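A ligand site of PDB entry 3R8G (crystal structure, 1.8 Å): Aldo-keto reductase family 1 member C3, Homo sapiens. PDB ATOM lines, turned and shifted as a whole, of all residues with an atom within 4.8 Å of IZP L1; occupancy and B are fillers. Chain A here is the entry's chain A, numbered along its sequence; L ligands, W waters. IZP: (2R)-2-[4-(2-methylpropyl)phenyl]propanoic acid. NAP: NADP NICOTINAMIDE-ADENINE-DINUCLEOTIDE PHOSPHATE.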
ATOM      1  N   LEU A  54     -25.826   1.016  29.099  1.00  0.00           N
ATOM      2  CA  LEU A  54     -25.110   1.668  30.212  1.00  0.00           C
ATOM      3  C   LEU A  54     -25.916   1.859  31.492  1.00  0.00           C
ATOM      4  O   LEU A  54     -25.351   1.846  32.594  1.00  0.00           O
ATOM      5  CB  LEU A  54     -24.633   3.069  29.767  1.00  0.00           C
ATOM      6  CG  LEU A  54     -23.617   3.762  30.680  1.00  0.00           C
ATOM      7  CD1 LEU A  54     -22.215   3.066  30.689  1.00  0.00           C
ATOM      8  CD2 LEU A  54     -23.377   5.210  30.149  1.00  0.00           C
ATOM      9  N   TYR A  55     -27.222   2.044  31.346  1.00  0.00           N
ATOM     10  CA  TYR A  55     -28.057   2.457  32.465  1.00  0.00           C
ATOM     11  C   TYR A  55     -28.375   1.343  33.454  1.00  0.00           C
ATOM     12  O   TYR A  55     -28.847   1.641  34.571  1.00  0.00           O
ATOM     13  CB  TYR A  55     -29.393   3.038  31.992  1.00  0.00           C
ATOM     14  CG  TYR A  55     -29.205   4.268  31.082  1.00  0.00           C
ATOM     15  CD1 TYR A  55     -27.958   4.895  30.976  1.00  0.00           C
ATOM     16  CD2 TYR A  55     -30.291   4.774  30.383  1.00  0.00           C
ATOM     17  CE1 TYR A  55     -27.780   6.023  30.068  1.00  0.00           C
ATOM     18  CE2 TYR A  55     -30.156   5.870  29.511  1.00  0.00           C
ATOM     19  CZ  TYR A  55     -28.923   6.495  29.391  1.00  0.00           C
ATOM     20  OH  TYR A  55     -28.747   7.579  28.568  1.00  0.00           O
ATOM     21  N   TRP A  86     -23.229   0.763  23.723  1.00  0.00           N
ATOM     22  CA  TRP A  86     -22.239   1.424  24.540  1.00  0.00           C
ATOM     23  C   TRP A  86     -20.895   1.399  23.789  1.00  0.00           C
ATOM     24  O   TRP A  86     -20.706   0.596  22.849  1.00  0.00           O
ATOM     25  CB  TRP A  86     -22.112   0.772  25.948  1.00  0.00           C
ATOM     26  CG  TRP A  86     -21.113   1.579  26.783  1.00  0.00           C
ATOM     27  CD1 TRP A  86     -19.912   1.104  27.300  1.00  0.00           C
ATOM     28  CD2 TRP A  86     -21.110   2.995  26.993  1.00  0.00           C
ATOM     29  NE1 TRP A  86     -19.192   2.142  27.881  1.00  0.00           N
ATOM     30  CE2 TRP A  86     -19.892   3.321  27.675  1.00  0.00           C
ATOM     31  CE3 TRP A  86     -22.004   4.025  26.670  1.00  0.00           C
ATOM     32  CZ2 TRP A  86     -19.595   4.633  28.083  1.00  0.00           C
ATOM     33  CZ3 TRP A  86     -21.690   5.327  27.005  1.00  0.00           C
ATOM     34  CH2 TRP A  86     -20.491   5.624  27.726  1.00  0.00           C
ATOM     35  N   HIS A 117     -24.339   5.250  21.228  1.00  0.00           N
ATOM     36  CA  HIS A 117     -24.492   6.096  22.412  1.00  0.00           C
ATOM     37  C   HIS A 117     -23.526   7.275  22.364  1.00  0.00           C
ATOM     38  O   HIS A 117     -23.869   8.390  22.832  1.00  0.00           O
ATOM     39  CB  HIS A 117     -24.183   5.266  23.698  1.00  0.00           C
ATOM     40  CG  HIS A 117     -24.754   5.839  24.962  1.00  0.00           C
ATOM     41  ND1 HIS A 117     -25.262   5.044  25.966  1.00  0.00           N
ATOM     42  CD2 HIS A 117     -24.882   7.124  25.392  1.00  0.00           C
ATOM     43  CE1 HIS A 117     -25.701   5.810  26.967  1.00  0.00           C
ATOM     44  NE2 HIS A 117     -25.488   7.068  26.633  1.00  0.00           N
ATOM     45  N   SER A 118     -22.358   7.058  21.775  1.00  0.00           N
ATOM     46  CA  SER A 118     -21.412   8.165  21.763  1.00  0.00           C
ATOM     47  C   SER A 118     -20.359   7.871  20.686  1.00  0.00           C
ATOM     48  O   SER A 118     -20.085   6.692  20.374  1.00  0.00           O
ATOM     49  CB  SER A 118     -20.788   8.232  23.193  1.00  0.00           C
ATOM     50  OG  SER A 118     -19.502   8.687  23.213  1.00  0.00           O
ATOM     51  N   MET A 120     -17.312   8.267  21.069  1.00  0.00           N
ATOM     52  CA  MET A 120     -16.006   8.104  21.745  1.00  0.00           C
ATOM     53  C   MET A 120     -15.691   6.651  22.055  1.00  0.00           C
ATOM     54  O   MET A 120     -16.005   6.151  23.117  1.00  0.00           O
ATOM     55  CB  MET A 120     -15.925   8.951  23.007  1.00  0.00           C
ATOM     56  CG  MET A 120     -15.983  10.454  22.712  1.00  0.00           C
ATOM     57  SD  MET A 120     -16.083  11.449  24.201  1.00  0.00           S
ATOM     58  CE  MET A 120     -17.818  11.144  24.654  1.00  0.00           C
ATOM     59  N   ASN A 167     -24.788  12.076  20.697  1.00  0.00           N
ATOM     60  CA  ASN A 167     -23.610  12.877  21.075  1.00  0.00           C
ATOM     61  C   ASN A 167     -22.654  13.090  19.877  1.00  0.00           C
ATOM     62  O   ASN A 167     -21.438  13.240  20.075  1.00  0.00           O
ATOM     63  CB  ASN A 167     -22.868  12.205  22.248  1.00  0.00           C
ATOM     64  CG  ASN A 167     -23.704  12.220  23.507  1.00  0.00           C
ATOM     65  OD1 ASN A 167     -24.083  13.298  23.918  1.00  0.00           O
ATOM     66  ND2 ASN A 167     -24.073  11.042  24.071  1.00  0.00           N
ATOM     67  N   TYR A 216     -31.525  15.567  25.466  1.00  0.00           N
ATOM     68  CA  TYR A 216     -31.421  15.074  26.851  1.00  0.00           C
ATOM     69  C   TYR A 216     -30.867  16.190  27.760  1.00  0.00           C
ATOM     70  O   TYR A 216     -30.350  17.223  27.291  1.00  0.00           O
ATOM     71  CB  TYR A 216     -30.563  13.803  26.958  1.00  0.00           C
ATOM     72  CG  TYR A 216     -29.061  13.969  26.714  1.00  0.00           C
ATOM     73  CD1 TYR A 216     -28.239  14.589  27.682  1.00  0.00           C
ATOM     74  CD2 TYR A 216     -28.447  13.439  25.572  1.00  0.00           C
ATOM     75  CE1 TYR A 216     -26.880  14.689  27.484  1.00  0.00           C
ATOM     76  CE2 TYR A 216     -27.034  13.498  25.413  1.00  0.00           C
ATOM     77  CZ  TYR A 216     -26.302  14.150  26.395  1.00  0.00           C
ATOM     78  OH  TYR A 216     -24.916  14.229  26.260  1.00  0.00           O
ATOM     79  N   TRP A 227     -19.805  13.905  36.816  1.00  0.00           N
ATOM     80  CA  TRP A 227     -19.559  14.642  35.587  1.00  0.00           C
ATOM     81  C   TRP A 227     -19.979  16.127  35.551  1.00  0.00           C
ATOM     82  O   TRP A 227     -19.543  16.848  34.651  1.00  0.00           O
ATOM     83  CB  TRP A 227     -20.347  13.958  34.452  1.00  0.00           C
ATOM     84  CG  TRP A 227     -20.182  12.489  34.399  1.00  0.00           C
ATOM     85  CD1 TRP A 227     -19.033  11.781  34.105  1.00  0.00           C
ATOM     86  CD2 TRP A 227     -21.175  11.545  34.700  1.00  0.00           C
ATOM     87  NE1 TRP A 227     -19.291  10.436  34.184  1.00  0.00           N
ATOM     88  CE2 TRP A 227     -20.595  10.262  34.559  1.00  0.00           C
ATOM     89  CE3 TRP A 227     -22.512  11.662  35.092  1.00  0.00           C
ATOM     90  CZ2 TRP A 227     -21.324   9.077  34.784  1.00  0.00           C
ATOM     91  CZ3 TRP A 227     -23.234  10.478  35.324  1.00  0.00           C
ATOM     92  CH2 TRP A 227     -22.630   9.204  35.157  1.00  0.00           C
ATOM     93  N   PHE A 306     -22.495  18.096  31.212  1.00  0.00           N
ATOM     94  CA  PHE A 306     -21.470  17.023  31.265  1.00  0.00           C
ATOM     95  C   PHE A 306     -20.126  17.572  30.874  1.00  0.00           C
ATOM     96  O   PHE A 306     -19.896  17.897  29.702  1.00  0.00           O
ATOM     97  CB  PHE A 306     -21.876  15.820  30.367  1.00  0.00           C
ATOM     98  CG  PHE A 306     -23.039  15.055  30.908  1.00  0.00           C
ATOM     99  CD1 PHE A 306     -22.851  13.879  31.653  1.00  0.00           C
ATOM    100  CD2 PHE A 306     -24.367  15.527  30.711  1.00  0.00           C
ATOM    101  CE1 PHE A 306     -23.943  13.165  32.168  1.00  0.00           C
ATOM    102  CE2 PHE A 306     -25.493  14.820  31.302  1.00  0.00           C
ATOM    103  CZ  PHE A 306     -25.276  13.652  31.987  1.00  0.00           C
ATOM    104  N   PHE A 311     -14.292  12.522  29.509  1.00  0.00           N
ATOM    105  CA  PHE A 311     -14.772  12.687  28.144  1.00  0.00           C
ATOM    106  C   PHE A 311     -13.816  13.618  27.404  1.00  0.00           C
ATOM    107  O   PHE A 311     -13.486  13.378  26.262  1.00  0.00           O
ATOM    108  CB  PHE A 311     -16.169  13.363  28.149  1.00  0.00           C
ATOM    109  CG  PHE A 311     -17.186  12.635  28.951  1.00  0.00           C
ATOM    110  CD1 PHE A 311     -17.620  11.356  28.561  1.00  0.00           C
ATOM    111  CD2 PHE A 311     -17.781  13.259  30.069  1.00  0.00           C
ATOM    112  CE1 PHE A 311     -18.634  10.676  29.321  1.00  0.00           C
ATOM    113  CE2 PHE A 311     -18.772  12.597  30.832  1.00  0.00           C
ATOM    114  CZ  PHE A 311     -19.194  11.299  30.462  1.00  0.00           C
ATOM    115  N   TYR A 317     -13.884  13.375  21.301  1.00  0.00           N
ATOM    116  CA  TYR A 317     -14.801  14.214  22.112  1.00  0.00           C
ATOM    117  C   TYR A 317     -15.613  15.151  21.203  1.00  0.00           C
ATOM    118  O   TYR A 317     -15.040  15.898  20.417  1.00  0.00           O
ATOM    119  CB  TYR A 317     -13.869  15.073  23.005  1.00  0.00           C
ATOM    120  CG  TYR A 317     -14.548  15.949  23.998  1.00  0.00           C
ATOM    121  CD1 TYR A 317     -15.501  15.414  24.883  1.00  0.00           C
ATOM    122  CD2 TYR A 317     -14.208  17.289  24.095  1.00  0.00           C
ATOM    123  CE1 TYR A 317     -16.109  16.213  25.862  1.00  0.00           C
ATOM    124  CE2 TYR A 317     -14.809  18.116  25.062  1.00  0.00           C
ATOM    125  CZ  TYR A 317     -15.753  17.547  25.945  1.00  0.00           C
ATOM    126  OH  TYR A 317     -16.335  18.301  26.936  1.00  0.00           O
ATOM    127  N   PRO A 318     -16.946  15.170  21.307  1.00  0.00           N
ATOM    128  CA  PRO A 318     -17.648  15.950  20.288  1.00  0.00           C
ATOM    129  C   PRO A 318     -17.582  17.442  20.534  1.00  0.00           C
ATOM    130  O   PRO A 318     -17.894  18.195  19.613  1.00  0.00           O
ATOM    131  CB  PRO A 318     -19.146  15.507  20.439  1.00  0.00           C
ATOM    132  CG  PRO A 318     -19.206  14.973  21.870  1.00  0.00           C
ATOM    133  CD  PRO A 318     -17.856  14.290  22.075  1.00  0.00           C
ATOM    134  N   TYR A 319     -17.264  17.882  21.752  1.00  0.00           N
ATOM    135  CA  TYR A 319     -17.341  19.295  21.973  1.00  0.00           C
ATOM    136  C   TYR A 319     -16.007  19.984  21.650  1.00  0.00           C
ATOM    137  O   TYR A 319     -15.877  21.185  21.919  1.00  0.00           O
ATOM    138  CB  TYR A 319     -17.714  19.600  23.421  1.00  0.00           C
ATOM    139  CG  TYR A 319     -19.077  19.019  23.811  1.00  0.00           C
ATOM    140  CD1 TYR A 319     -20.123  19.081  22.917  1.00  0.00           C
ATOM    141  CD2 TYR A 319     -19.270  18.462  25.064  1.00  0.00           C
ATOM    142  CE1 TYR A 319     -21.375  18.527  23.259  1.00  0.00           C
ATOM    143  CE2 TYR A 319     -20.503  17.948  25.437  1.00  0.00           C
ATOM    144  CZ  TYR A 319     -21.551  17.994  24.519  1.00  0.00           C
ATOM    145  OH  TYR A 319     -22.779  17.460  24.905  1.00  0.00           O
HETATM  146  C1  IZP L   1     -25.379   8.854  29.886  1.00  0.00           C
HETATM  147  O1  IZP L   1     -26.172   8.433  28.948  1.00  0.00           O
HETATM  148  C2  IZP L   1     -21.510  12.721  26.103  1.00  0.00           C
HETATM  149  O2  IZP L   1     -25.777   9.183  31.007  1.00  0.00           O
HETATM  150  C3  IZP L   1     -20.169  13.334  26.439  1.00  0.00           C
HETATM  151  C4  IZP L   1     -19.702  14.101  25.208  1.00  0.00           C
HETATM  152  C5  IZP L   1     -20.288  14.325  27.586  1.00  0.00           C
HETATM  153  C6  IZP L   1     -23.854   8.794  29.738  1.00  0.00           C
HETATM  154  C7  IZP L   1     -23.100   8.968  31.114  1.00  0.00           C
HETATM  155  C8  IZP L   1     -23.270   9.847  28.805  1.00  0.00           C
HETATM  156  C9  IZP L   1     -23.480  11.230  29.054  1.00  0.00           C
HETATM  157  C10 IZP L   1     -22.904  12.111  28.122  1.00  0.00           C
HETATM  158  C11 IZP L   1     -22.098  11.691  27.063  1.00  0.00           C
HETATM  159  C12 IZP L   1     -21.846  10.326  26.885  1.00  0.00           C
HETATM  160  C13 IZP L   1     -22.464   9.392  27.754  1.00  0.00           C
HETATM  161  PA  NAP L   2     -33.508  15.692  32.888  1.00  0.00           P
HETATM  162  O1A NAP L   2     -32.637  16.849  32.493  1.00  0.00           O
HETATM  163  O2A NAP L   2     -34.564  15.292  31.955  1.00  0.00           O
HETATM  164  O5B NAP L   2     -34.017  15.961  34.410  1.00  0.00           O
HETATM  165  C5B NAP L   2     -33.162  16.554  35.437  1.00  0.00           C
HETATM  166  C4B NAP L   2     -33.971  16.508  36.797  1.00  0.00           C
HETATM  167  O4B NAP L   2     -35.152  17.181  36.538  1.00  0.00           O
HETATM  168  C3B NAP L   2     -34.443  15.064  37.116  1.00  0.00           C
HETATM  169  O3B NAP L   2     -33.440  14.426  37.942  1.00  0.00           O
HETATM  170  C2B NAP L   2     -35.803  15.246  37.793  1.00  0.00           C
HETATM  171  O2B NAP L   2     -35.728  14.985  39.175  1.00  0.00           O
HETATM  172  C1B NAP L   2     -36.012  16.720  37.587  1.00  0.00           C
HETATM  173  N9A NAP L   2     -37.444  17.028  37.082  1.00  0.00           N
HETATM  174  C8A NAP L   2     -38.116  16.249  36.210  1.00  0.00           C
HETATM  175  N7A NAP L   2     -39.308  16.797  36.031  1.00  0.00           N
HETATM  176  C5A NAP L   2     -39.400  17.903  36.808  1.00  0.00           C
HETATM  177  C6A NAP L   2     -40.405  18.848  37.050  1.00  0.00           C
HETATM  178  N6A NAP L   2     -41.610  18.807  36.428  1.00  0.00           N
HETATM  179  N1A NAP L   2     -40.103  19.824  37.972  1.00  0.00           N
HETATM  180  C2A NAP L   2     -38.895  19.935  38.562  1.00  0.00           C
HETATM  181  N3A NAP L   2     -37.914  19.055  38.389  1.00  0.00           N
HETATM  182  C4A NAP L   2     -38.171  18.057  37.470  1.00  0.00           C
HETATM  183  O3  NAP L   2     -32.451  14.509  33.162  1.00  0.00           O
HETATM  184  PN  NAP L   2     -31.327  13.657  32.373  1.00  0.00           P
HETATM  185  O1N NAP L   2     -30.065  14.464  32.244  1.00  0.00           O
HETATM  186  O2N NAP L   2     -31.245  12.337  32.997  1.00  0.00           O
HETATM  187  O5D NAP L   2     -31.887  13.539  30.903  1.00  0.00           O
HETATM  188  C5D NAP L   2     -33.097  12.736  30.660  1.00  0.00           C
HETATM  189  C4D NAP L   2     -32.795  11.327  30.048  1.00  0.00           C
HETATM  190  O4D NAP L   2     -32.017  11.613  28.800  1.00  0.00           O
HETATM  191  C3D NAP L   2     -31.944  10.368  30.864  1.00  0.00           C
HETATM  192  O3D NAP L   2     -32.778   9.804  31.923  1.00  0.00           O
HETATM  193  C2D NAP L   2     -31.536   9.405  29.762  1.00  0.00           C
HETATM  194  O2D NAP L   2     -32.678   8.630  29.371  1.00  0.00           O
HETATM  195  C1D NAP L   2     -31.203  10.436  28.585  1.00  0.00           C
HETATM  196  N1N NAP L   2     -29.785  10.843  28.581  1.00  0.00           N
HETATM  197  C2N NAP L   2     -29.047  10.385  27.513  1.00  0.00           C
HETATM  198  C3N NAP L   2     -27.674  10.714  27.412  1.00  0.00           C
HETATM  199  C7N NAP L   2     -26.888  10.310  26.197  1.00  0.00           C
HETATM  200  O7N NAP L   2     -25.647  10.325  26.253  1.00  0.00           O
HETATM  201  N7N NAP L   2     -27.636  10.019  25.086  1.00  0.00           N
HETATM  202  C4N NAP L   2     -27.060  11.444  28.412  1.00  0.00           C
HETATM  203  C5N NAP L   2     -27.859  11.931  29.492  1.00  0.00           C
HETATM  204  C6N NAP L   2     -29.221  11.645  29.587  1.00  0.00           C
HETATM  205  P2B NAP L   2     -36.858  13.967  39.821  1.00  0.00           P
HETATM  206  O1X NAP L   2     -38.244  14.501  39.395  1.00  0.00           O
HETATM  207  O2X NAP L   2     -36.501  14.187  41.406  1.00  0.00           O
HETATM  208  O3X NAP L   2     -36.464  12.570  39.415  1.00  0.00           O
HETATM  209  O   HOH W   1     -28.214   9.346  31.433  1.00  0.00           O
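Leu 54 touches IZP L1. CE of Met 120 touches C4 of IZP L1 (3.5 Å). Asn 167 touches IZP L1 (OD1 to C2, 3.4 Å). OH of Tyr 216 touches C10 of IZP L1 (3.5 Å). Phe 306 touches IZP L1. Phe 311 touches IZP L1 (CD2 to C5, 3.7 Å). Pro 318 touches IZP L1. Tyr 319 touches IZP L1. Hydrophobic or aromatic side chains that line IZP L1: Leu 54, Tyr 55, His 117, Met 120, Phe 306, Phe 311, Pro 318 and Tyr 319. Within 4 Å of IZP L1: Leu 54, Tyr 55, His 117, Met 120, Asn 167, Tyr 216, Phe 306, Phe 311, Pro 318 and Tyr 319. The nearest printed residue that does not touch IZP L1 is Trp 227 (4.1 Å).
OH of Tyr 55 is in hydrogen-bond range of O1 of IZP L1 (2.7 Å). An oxygen (O1) of IZP L1 lies within hydrogen-bond range of a ring nitrogen (NE2) of His 117 (2.8 Å). A ring nitrogen (NE2) of His 117 sits at hydrogen-bond distance from an oxygen (O7N) of NAP L2 (3.3 Å). An oxygen (O7N) of NAP L2 sits at hydrogen-bond distance from the side-chain amide nitrogen (ND2) of Asn 167, 2.8 Å away.
Water W1 bridges O2 of IZP L1 (2.5 Å) and OH of Tyr 55 (3.4 Å).
O of His 117 sits at hydrogen-bond distance from ND2 of Asn 167 (2.9 Å). The side-chain amide oxygen (OD1) of Asn 167 sits at hydrogen-bond distance from the side-chain hydroxyl (OH) of Tyr 216 (2.7 Å). N of Met 120 lies within hydrogen-bond range of OG of Ser 118, at 3.1 Å.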
